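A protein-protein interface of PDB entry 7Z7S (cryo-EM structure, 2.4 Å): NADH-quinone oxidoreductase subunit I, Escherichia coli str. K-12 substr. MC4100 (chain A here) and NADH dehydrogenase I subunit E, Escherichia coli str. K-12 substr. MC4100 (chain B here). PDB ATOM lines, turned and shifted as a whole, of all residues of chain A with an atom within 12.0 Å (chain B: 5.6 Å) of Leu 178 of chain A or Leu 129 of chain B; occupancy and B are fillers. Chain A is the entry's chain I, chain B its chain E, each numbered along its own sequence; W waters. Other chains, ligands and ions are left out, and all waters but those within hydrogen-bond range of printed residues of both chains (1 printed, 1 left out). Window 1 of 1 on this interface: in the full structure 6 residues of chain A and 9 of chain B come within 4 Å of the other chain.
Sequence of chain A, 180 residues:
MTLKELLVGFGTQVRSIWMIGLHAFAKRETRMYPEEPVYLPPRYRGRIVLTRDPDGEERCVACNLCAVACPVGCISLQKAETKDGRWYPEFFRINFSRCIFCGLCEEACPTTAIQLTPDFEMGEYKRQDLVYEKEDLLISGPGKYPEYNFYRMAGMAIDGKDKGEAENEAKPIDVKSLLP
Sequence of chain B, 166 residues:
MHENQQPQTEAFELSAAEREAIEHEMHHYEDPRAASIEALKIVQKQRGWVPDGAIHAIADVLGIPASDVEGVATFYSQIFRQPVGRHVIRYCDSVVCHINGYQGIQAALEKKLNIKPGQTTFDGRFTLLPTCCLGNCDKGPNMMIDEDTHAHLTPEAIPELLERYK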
ATOM      1  N   PRO A 172     -29.521  11.925 -25.447  1.00  0.00           N
ATOM      2  CA  PRO A 172     -28.881  12.541 -26.612  1.00  0.00           C
ATOM      3  C   PRO A 172     -27.883  13.609 -26.206  1.00  0.00           C
ATOM      4  O   PRO A 172     -28.111  14.382 -25.274  1.00  0.00           O
ATOM      5  CB  PRO A 172     -30.058  13.138 -27.392  1.00  0.00           C
ATOM      6  CG  PRO A 172     -31.141  13.272 -26.403  1.00  0.00           C
ATOM      7  CD  PRO A 172     -30.972  12.160 -25.430  1.00  0.00           C
ATOM      8  N   ILE A 173     -26.760  13.632 -26.911  1.00  0.00           N
ATOM      9  CA  ILE A 173     -25.699  14.604 -26.693  1.00  0.00           C
ATOM     10  C   ILE A 173     -25.710  15.552 -27.875  1.00  0.00           C
ATOM     11  O   ILE A 173     -25.591  15.117 -29.026  1.00  0.00           O
ATOM     12  CB  ILE A 173     -24.329  13.929 -26.542  1.00  0.00           C
ATOM     13  CG1 ILE A 173     -24.346  12.926 -25.391  1.00  0.00           C
ATOM     14  CG2 ILE A 173     -23.243  14.967 -26.347  1.00  0.00           C
ATOM     15  CD1 ILE A 173     -23.111  12.071 -25.325  1.00  0.00           C
ATOM     16  N   ASP A 174     -25.867  16.841 -27.598  1.00  0.00           N
ATOM     17  CA  ASP A 174     -25.806  17.835 -28.654  1.00  0.00           C
ATOM     18  C   ASP A 174     -24.388  17.931 -29.198  1.00  0.00           C
ATOM     19  O   ASP A 174     -23.410  17.734 -28.475  1.00  0.00           O
ATOM     20  CB  ASP A 174     -26.262  19.195 -28.133  1.00  0.00           C
ATOM     21  CG  ASP A 174     -26.794  20.088 -29.234  1.00  0.00           C
ATOM     22  OD1 ASP A 174     -25.985  20.768 -29.888  1.00  0.00           O
ATOM     23  OD2 ASP A 174     -28.022  20.110 -29.446  1.00  0.00           O
ATOM     24  N   VAL A 175     -24.279  18.225 -30.497  1.00  0.00           N
ATOM     25  CA  VAL A 175     -22.959  18.387 -31.098  1.00  0.00           C
ATOM     26  C   VAL A 175     -22.279  19.663 -30.625  1.00  0.00           C
ATOM     27  O   VAL A 175     -21.064  19.807 -30.781  1.00  0.00           O
ATOM     28  CB  VAL A 175     -23.037  18.361 -32.636  1.00  0.00           C
ATOM     29  CG1 VAL A 175     -23.475  16.998 -33.116  1.00  0.00           C
ATOM     30  CG2 VAL A 175     -23.969  19.447 -33.150  1.00  0.00           C
ATOM     31  N   LYS A 176     -23.027  20.586 -30.035  1.00  0.00           N
ATOM     32  CA  LYS A 176     -22.485  21.815 -29.483  1.00  0.00           C
ATOM     33  C   LYS A 176     -22.019  21.666 -28.043  1.00  0.00           C
ATOM     34  O   LYS A 176     -21.630  22.664 -27.433  1.00  0.00           O
ATOM     35  CB  LYS A 176     -23.526  22.927 -29.571  1.00  0.00           C
ATOM     36  CG  LYS A 176     -24.046  23.164 -30.970  1.00  0.00           C
ATOM     37  CD  LYS A 176     -24.598  24.561 -31.127  1.00  0.00           C
ATOM     38  CE  LYS A 176     -26.110  24.572 -31.149  1.00  0.00           C
ATOM     39  NZ  LYS A 176     -26.688  24.024 -29.896  1.00  0.00           N
ATOM     40  N   SER A 177     -22.053  20.458 -27.491  1.00  0.00           N
ATOM     41  CA  SER A 177     -21.660  20.237 -26.107  1.00  0.00           C
ATOM     42  C   SER A 177     -20.170  20.490 -25.911  1.00  0.00           C
ATOM     43  O   SER A 177     -19.349  20.225 -26.788  1.00  0.00           O
ATOM     44  CB  SER A 177     -22.002  18.812 -25.678  1.00  0.00           C
ATOM     45  OG  SER A 177     -20.967  17.916 -26.026  1.00  0.00           O
ATOM     46  N   LEU A 178     -19.831  21.016 -24.733  1.00  0.00           N
ATOM     47  CA  LEU A 178     -18.458  21.412 -24.449  1.00  0.00           C
ATOM     48  C   LEU A 178     -17.545  20.229 -24.180  1.00  0.00           C
ATOM     49  O   LEU A 178     -16.328  20.361 -24.335  1.00  0.00           O
ATOM     50  CB  LEU A 178     -18.421  22.365 -23.259  1.00  0.00           C
ATOM     51  CG  LEU A 178     -19.326  23.588 -23.346  1.00  0.00           C
ATOM     52  CD1 LEU A 178     -19.421  24.267 -21.996  1.00  0.00           C
ATOM     53  CD2 LEU A 178     -18.815  24.548 -24.399  1.00  0.00           C
ATOM     54  N   LEU A 179     -18.093  19.092 -23.774  1.00  0.00           N
ATOM     55  CA  LEU A 179     -17.263  17.933 -23.488  1.00  0.00           C
ATOM     56  C   LEU A 179     -16.701  17.358 -24.787  1.00  0.00           C
ATOM     57  O   LEU A 179     -17.414  17.283 -25.789  1.00  0.00           O
ATOM     58  CB  LEU A 179     -18.067  16.871 -22.746  1.00  0.00           C
ATOM     59  CG  LEU A 179     -18.413  17.229 -21.301  1.00  0.00           C
ATOM     60  CD1 LEU A 179     -19.456  16.286 -20.742  1.00  0.00           C
ATOM     61  CD2 LEU A 179     -17.166  17.211 -20.447  1.00  0.00           C
ATOM     62  N   PRO A 180     -15.423  16.951 -24.801  1.00  0.00           N
ATOM     63  CA  PRO A 180     -14.766  16.402 -25.993  1.00  0.00           C
ATOM     64  C   PRO A 180     -15.349  15.061 -26.443  1.00  0.00           C
ATOM     65  O   PRO A 180     -15.970  14.357 -25.645  1.00  0.00           O
ATOM     66  CB  PRO A 180     -13.310  16.229 -25.547  1.00  0.00           C
ATOM     67  CG  PRO A 180     -13.170  17.047 -24.313  1.00  0.00           C
ATOM     68  CD  PRO A 180     -14.501  17.021 -23.657  1.00  0.00           C
ATOM     69  N   SER B  77     -12.814  20.771 -30.503  1.00  0.00           N
ATOM     70  CA  SER B  77     -13.266  20.777 -29.120  1.00  0.00           C
ATOM     71  C   SER B  77     -13.050  22.124 -28.444  1.00  0.00           C
ATOM     72  O   SER B  77     -13.790  22.470 -27.520  1.00  0.00           O
ATOM     73  CB  SER B  77     -12.565  19.668 -28.340  1.00  0.00           C
ATOM     74  OG  SER B  77     -11.163  19.757 -28.469  1.00  0.00           O
ATOM     75  N   PHE B  80     -16.079  26.752 -28.720  1.00  0.00           N
ATOM     76  CA  PHE B  80     -17.218  26.544 -27.839  1.00  0.00           C
ATOM     77  C   PHE B  80     -18.484  27.050 -28.511  1.00  0.00           C
ATOM     78  O   PHE B  80     -18.583  28.230 -28.859  1.00  0.00           O
ATOM     79  CB  PHE B  80     -16.993  27.244 -26.502  1.00  0.00           C
ATOM     80  CG  PHE B  80     -15.761  26.788 -25.788  1.00  0.00           C
ATOM     81  CD1 PHE B  80     -15.432  25.448 -25.744  1.00  0.00           C
ATOM     82  CD2 PHE B  80     -14.927  27.697 -25.169  1.00  0.00           C
ATOM     83  CE1 PHE B  80     -14.301  25.023 -25.094  1.00  0.00           C
ATOM     84  CE2 PHE B  80     -13.793  27.276 -24.517  1.00  0.00           C
ATOM     85  CZ  PHE B  80     -13.483  25.936 -24.478  1.00  0.00           C
ATOM     86  N   ARG B  81     -19.443  26.155 -28.704  1.00  0.00           N
ATOM     87  CA  ARG B  81     -20.734  26.501 -29.269  1.00  0.00           C
ATOM     88  C   ARG B  81     -21.823  26.551 -28.212  1.00  0.00           C
ATOM     89  O   ARG B  81     -23.006  26.608 -28.551  1.00  0.00           O
ATOM     90  CB  ARG B  81     -21.097  25.515 -30.375  1.00  0.00           C
ATOM     91  CG  ARG B  81     -20.329  25.735 -31.657  1.00  0.00           C
ATOM     92  CD  ARG B  81     -20.739  27.026 -32.321  1.00  0.00           C
ATOM     93  NE  ARG B  81     -22.018  26.886 -33.001  1.00  0.00           N
ATOM     94  CZ  ARG B  81     -23.144  27.458 -32.602  1.00  0.00           C
ATOM     95  NH1 ARG B  81     -23.182  28.242 -31.541  1.00  0.00           N
ATOM     96  NH2 ARG B  81     -24.260  27.236 -33.286  1.00  0.00           N
ATOM     97  N   GLN B  82     -21.445  26.511 -26.941  1.00  0.00           N
ATOM     98  CA  GLN B  82     -22.309  26.729 -25.797  1.00  0.00           C
ATOM     99  C   GLN B  82     -21.639  27.745 -24.889  1.00  0.00           C
ATOM    100  O   GLN B  82     -20.407  27.826 -24.861  1.00  0.00           O
ATOM    101  CB  GLN B  82     -22.564  25.424 -25.030  1.00  0.00           C
ATOM    102  CG  GLN B  82     -23.670  24.580 -25.616  1.00  0.00           C
ATOM    103  CD  GLN B  82     -23.745  23.211 -24.989  1.00  0.00           C
ATOM    104  OE1 GLN B  82     -23.019  22.912 -24.043  1.00  0.00           O
ATOM    105  NE2 GLN B  82     -24.618  22.365 -25.515  1.00  0.00           N
ATOM    106  N   PRO B  83     -22.414  28.557 -24.167  1.00  0.00           N
ATOM    107  CA  PRO B  83     -21.805  29.582 -23.312  1.00  0.00           C
ATOM    108  C   PRO B  83     -20.997  28.973 -22.179  1.00  0.00           C
ATOM    109  O   PRO B  83     -21.388  27.975 -21.573  1.00  0.00           O
ATOM    110  CB  PRO B  83     -23.011  30.364 -22.781  1.00  0.00           C
ATOM    111  CG  PRO B  83     -24.161  29.457 -22.953  1.00  0.00           C
ATOM    112  CD  PRO B  83     -23.881  28.666 -24.179  1.00  0.00           C
ATOM    113  N   VAL B  84     -19.851  29.588 -21.903  1.00  0.00           N
ATOM    114  CA  VAL B  84     -18.955  29.113 -20.858  1.00  0.00           C
ATOM    115  C   VAL B  84     -18.815  30.193 -19.797  1.00  0.00           C
ATOM    116  O   VAL B  84     -19.403  31.273 -19.913  1.00  0.00           O
ATOM    117  CB  VAL B  84     -17.583  28.723 -21.434  1.00  0.00           C
ATOM    118  CG1 VAL B  84     -17.736  27.617 -22.455  1.00  0.00           C
ATOM    119  CG2 VAL B  84     -16.911  29.927 -22.053  1.00  0.00           C
ATOM    120  N   VAL B  88     -11.996  29.252 -18.208  1.00  0.00           N
ATOM    121  CA  VAL B  88     -12.171  27.856 -18.578  1.00  0.00           C
ATOM    122  C   VAL B  88     -11.002  27.080 -17.994  1.00  0.00           C
ATOM    123  O   VAL B  88      -9.850  27.275 -18.390  1.00  0.00           O
ATOM    124  CB  VAL B  88     -12.263  27.682 -20.099  1.00  0.00           C
ATOM    125  CG1 VAL B  88     -12.487  26.229 -20.454  1.00  0.00           C
ATOM    126  CG2 VAL B  88     -13.380  28.536 -20.655  1.00  0.00           C
ATOM    127  N   ILE B  89     -11.295  26.215 -17.036  1.00  0.00           N
ATOM    128  CA  ILE B  89     -10.314  25.301 -16.476  1.00  0.00           C
ATOM    129  C   ILE B  89     -10.300  24.046 -17.328  1.00  0.00           C
ATOM    130  O   ILE B  89     -11.350  23.452 -17.585  1.00  0.00           O
ATOM    131  CB  ILE B  89     -10.648  24.967 -15.017  1.00  0.00           C
ATOM    132  CG1 ILE B  89     -10.896  26.247 -14.230  1.00  0.00           C
ATOM    133  CG2 ILE B  89      -9.544  24.150 -14.395  1.00  0.00           C
ATOM    134  CD1 ILE B  89     -11.398  25.997 -12.862  1.00  0.00           C
ATOM    135  N   ARG B  90      -9.119  23.651 -17.783  1.00  0.00           N
ATOM    136  CA  ARG B  90      -8.970  22.473 -18.629  1.00  0.00           C
ATOM    137  C   ARG B  90      -7.948  21.556 -17.976  1.00  0.00           C
ATOM    138  O   ARG B  90      -6.742  21.744 -18.141  1.00  0.00           O
ATOM    139  CB  ARG B  90      -8.556  22.859 -20.041  1.00  0.00           C
ATOM    140  CG  ARG B  90      -9.723  23.266 -20.902  1.00  0.00           C
ATOM    141  CD  ARG B  90      -9.340  23.335 -22.351  1.00  0.00           C
ATOM    142  NE  ARG B  90      -8.165  24.164 -22.568  1.00  0.00           N
ATOM    143  CZ  ARG B  90      -8.209  25.421 -22.982  1.00  0.00           C
ATOM    144  NH1 ARG B  90      -9.359  26.023 -23.235  1.00  0.00           N
ATOM    145  NH2 ARG B  90      -7.073  26.094 -23.137  1.00  0.00           N
ATOM    146  N   TYR B  91      -8.428  20.566 -17.238  1.00  0.00           N
ATOM    147  CA  TYR B  91      -7.532  19.629 -16.579  1.00  0.00           C
ATOM    148  C   TYR B  91      -7.262  18.448 -17.496  1.00  0.00           C
ATOM    149  O   TYR B  91      -8.170  17.938 -18.154  1.00  0.00           O
ATOM    150  CB  TYR B  91      -8.101  19.162 -15.234  1.00  0.00           C
ATOM    151  CG  TYR B  91      -9.336  18.293 -15.317  1.00  0.00           C
ATOM    152  CD1 TYR B  91     -10.597  18.861 -15.392  1.00  0.00           C
ATOM    153  CD2 TYR B  91      -9.240  16.909 -15.311  1.00  0.00           C
ATOM    154  CE1 TYR B  91     -11.722  18.079 -15.468  1.00  0.00           C
ATOM    155  CE2 TYR B  91     -10.359  16.122 -15.393  1.00  0.00           C
ATOM    156  CZ  TYR B  91     -11.598  16.713 -15.469  1.00  0.00           C
ATOM    157  OH  TYR B  91     -12.721  15.929 -15.546  1.00  0.00           O
ATOM    158  N   PRO B 117     -17.624  18.065 -14.471  1.00  0.00           N
ATOM    159  CA  PRO B 117     -16.966  18.428 -15.732  1.00  0.00           C
ATOM    160  C   PRO B 117     -17.975  18.717 -16.833  1.00  0.00           C
ATOM    161  O   PRO B 117     -19.003  18.051 -16.953  1.00  0.00           O
ATOM    162  CB  PRO B 117     -16.119  17.197 -16.053  1.00  0.00           C
ATOM    163  CG  PRO B 117     -15.840  16.603 -14.740  1.00  0.00           C
ATOM    164  CD  PRO B 117     -17.049  16.834 -13.904  1.00  0.00           C
ATOM    165  N   GLY B 118     -17.666  19.724 -17.641  1.00  0.00           N
ATOM    166  CA  GLY B 118     -18.584  20.203 -18.647  1.00  0.00           C
ATOM    167  C   GLY B 118     -19.610  21.190 -18.148  1.00  0.00           C
ATOM    168  O   GLY B 118     -20.422  21.669 -18.950  1.00  0.00           O
ATOM    169  N   THR B 120     -20.728  24.759 -15.687  1.00  0.00           N
ATOM    170  CA  THR B 120     -20.292  26.108 -15.365  1.00  0.00           C
ATOM    171  C   THR B 120     -20.857  26.471 -13.998  1.00  0.00           C
ATOM    172  O   THR B 120     -22.010  26.151 -13.697  1.00  0.00           O
ATOM    173  CB  THR B 120     -20.759  27.091 -16.461  1.00  0.00           C
ATOM    174  OG1 THR B 120     -19.881  26.999 -17.586  1.00  0.00           O
ATOM    175  CG2 THR B 120     -20.762  28.532 -15.983  1.00  0.00           C
ATOM    176  N   THR B 127     -15.683  27.413 -15.838  1.00  0.00           N
ATOM    177  CA  THR B 127     -16.200  26.262 -16.566  1.00  0.00           C
ATOM    178  C   THR B 127     -15.157  25.161 -16.467  1.00  0.00           C
ATOM    179  O   THR B 127     -14.019  25.347 -16.899  1.00  0.00           O
ATOM    180  CB  THR B 127     -16.488  26.604 -18.028  1.00  0.00           C
ATOM    181  OG1 THR B 127     -17.681  27.387 -18.107  1.00  0.00           O
ATOM    182  CG2 THR B 127     -16.686  25.342 -18.842  1.00  0.00           C
ATOM    183  N   LEU B 128     -15.540  24.024 -15.901  1.00  0.00           N
ATOM    184  CA  LEU B 128     -14.617  22.915 -15.708  1.00  0.00           C
ATOM    185  C   LEU B 128     -14.709  21.959 -16.888  1.00  0.00           C
ATOM    186  O   LEU B 128     -15.806  21.546 -17.273  1.00  0.00           O
ATOM    187  CB  LEU B 128     -14.929  22.182 -14.405  1.00  0.00           C
ATOM    188  CG  LEU B 128     -14.022  21.017 -14.034  1.00  0.00           C
ATOM    189  CD1 LEU B 128     -12.616  21.505 -13.776  1.00  0.00           C
ATOM    190  CD2 LEU B 128     -14.574  20.298 -12.827  1.00  0.00           C
ATOM    191  N   LEU B 129     -13.557  21.599 -17.454  1.00  0.00           N
ATOM    192  CA  LEU B 129     -13.525  20.762 -18.630  1.00  0.00           C
ATOM    193  C   LEU B 129     -12.338  19.809 -18.574  1.00  0.00           C
ATOM    194  O   LEU B 129     -11.209  20.236 -18.256  1.00  0.00           O
ATOM    195  CB  LEU B 129     -13.452  21.614 -19.899  1.00  0.00           C
ATOM    196  CG  LEU B 129     -14.762  22.162 -20.459  1.00  0.00           C
ATOM    197  CD1 LEU B 129     -14.479  23.135 -21.579  1.00  0.00           C
ATOM    198  CD2 LEU B 129     -15.653  21.037 -20.936  1.00  0.00           C
ATOM    199  N   PRO B 130     -12.550  18.530 -18.857  1.00  0.00           N
ATOM    200  CA  PRO B 130     -11.421  17.654 -19.150  1.00  0.00           C
ATOM    201  C   PRO B 130     -10.859  17.980 -20.518  1.00  0.00           C
ATOM    202  O   PRO B 130     -11.569  18.419 -21.422  1.00  0.00           O
ATOM    203  CB  PRO B 130     -12.040  16.256 -19.121  1.00  0.00           C
ATOM    204  CG  PRO B 130     -13.448  16.481 -19.529  1.00  0.00           C
ATOM    205  CD  PRO B 130     -13.839  17.834 -18.996  1.00  0.00           C
ATOM    206  N   THR B 131      -9.561  17.768 -20.661  1.00  0.00           N
ATOM    207  CA  THR B 131      -8.904  17.955 -21.937  1.00  0.00           C
ATOM    208  C   THR B 131      -7.922  16.819 -22.133  1.00  0.00           C
ATOM    209  O   THR B 131      -7.495  16.169 -21.179  1.00  0.00           O
ATOM    210  CB  THR B 131      -8.188  19.312 -22.031  1.00  0.00           C
ATOM    211  OG1 THR B 131      -7.617  19.460 -23.335  1.00  0.00           O
ATOM    212  CG2 THR B 131      -7.090  19.428 -20.996  1.00  0.00           C
HETATM  213  O   HOH W   1     -18.889  23.406 -28.018  1.00  0.00           O
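The backbone carbonyl oxygen (O) of Ile 89 of chain B lies within hydrogen-bond range of the backbone NH (N) of Leu 129 of chain B (2.9 Å). The backbone carbonyl oxygen of Leu 129 of chain B is in hydrogen-bond range of the backbone NH of Tyr 91 of chain B (3.0 Å). The backbone NH of Gly 118 of chain B lies within hydrogen-bond range of the backbone carbonyl oxygen of Leu 128 of chain B, at 2.6 Å. NZ of Lys 176 of chain A is in salt-bridge range of OD1 of Asp 174 of chain A (3.3 Å). The side-chain hydroxyl of Ser 177 of chain A lies close to the backbone carbonyl oxygen of Asp 174 of chain A (3.5 Å).
Printed residues of chain B within 4 Å of Lys 176 of chain A: Arg 81 (3.5 Å) and Gln 82 (3.3 Å). Leu 178 of chain A touches four residues of chain B. Of the printed residues of chain B, Leu 179 of chain A touches Pro 117, Gly 118 and Pro 130. Printed residues of chain B within 4 Å of Pro 180 of chain A: Pro 130 (3.6 Å). Ser 77 of chain B touches none of the printed residues of chain A. Of chain A, only Leu 178 (3.8 Å) comes within 4 Å of Phe 80 of chain B. Of the printed residues of chain A, Arg 81 of chain B touches Lys 176. Gln 82 of chain B touches just these residues of chain A: Lys 176 (3.3 Å), Ser 177 (3.6 Å) and Leu 178 (3.7 Å). No residue of chain A comes within 4 Å of Pro 83 of chain B. No residue of chain A comes within 4 Å of Val 88 of chain B. No residue of chain A comes within 4 Å of Ile 89 of chain B. No residue of chain A comes within 4 Å of Tyr 91 of chain B. Printed residues of chain A within 4 Å of Gly 118 of chain B: Leu 179 (3.8 Å). Thr 120 of chain B touches none of the printed residues of chain A. No residue of chain A comes within 4 Å of Thr 127 of chain B. No residue of chain A comes within 4 Å of Leu 128 of chain B. Leu 129 of chain B touches one residue of chain A. No residue of chain A comes within 4 Å of Thr 131 of chain B.
Printed residues of chain A that touch a printed residue of chain B: Lys 176, Ser 177, Leu 178, Leu 179 and Pro 180. Hydrophobic or aromatic side chains of chain B within 4 Å of the printed part of chain A: Phe 80, Val 84, Leu 129 and Pro 130. Among the printed residues, 11 pairs touch across the chains.
Water W1 lies within hydrogen-bond range of the backbone NH of Arg 81 of chain B (2.9 Å), the backbone carbonyl oxygen of Lys 176 of chain A (2.9 Å) and the backbone carbonyl oxygen of Ser 177 of chain A (3.4 Å).
Gln 82 of chain B touches Lys 176 of chain A. Ser 177 of chain A touches Gln 82 of chain B (CA to OE1, 3.6 Å). CD2 of Leu 178 of chain A touches CD1 of Phe 80 of chain B, 3.8 Å away. Leu 178 of chain A touches Gln 82 of chain B. CG1 of Val 84 of chain B touches CD1 of Leu 178 of chain A (3.8 Å). Leu 178 of chain A touches Leu 129 of chain B (O to CD2, 3.5 Å). Leu 179 of chain A touches Pro 117 of chain B (CD2 to C, 3.998 Å). CA of Gly 118 of chain B touches CD2 of Leu 179 of chain A, at 3.8 Å. Leu 179 of chain A touches Pro 130 of chain B. O of Pro 130 of chain B touches CG of Pro 180 of chain A, 3.6 Å away.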
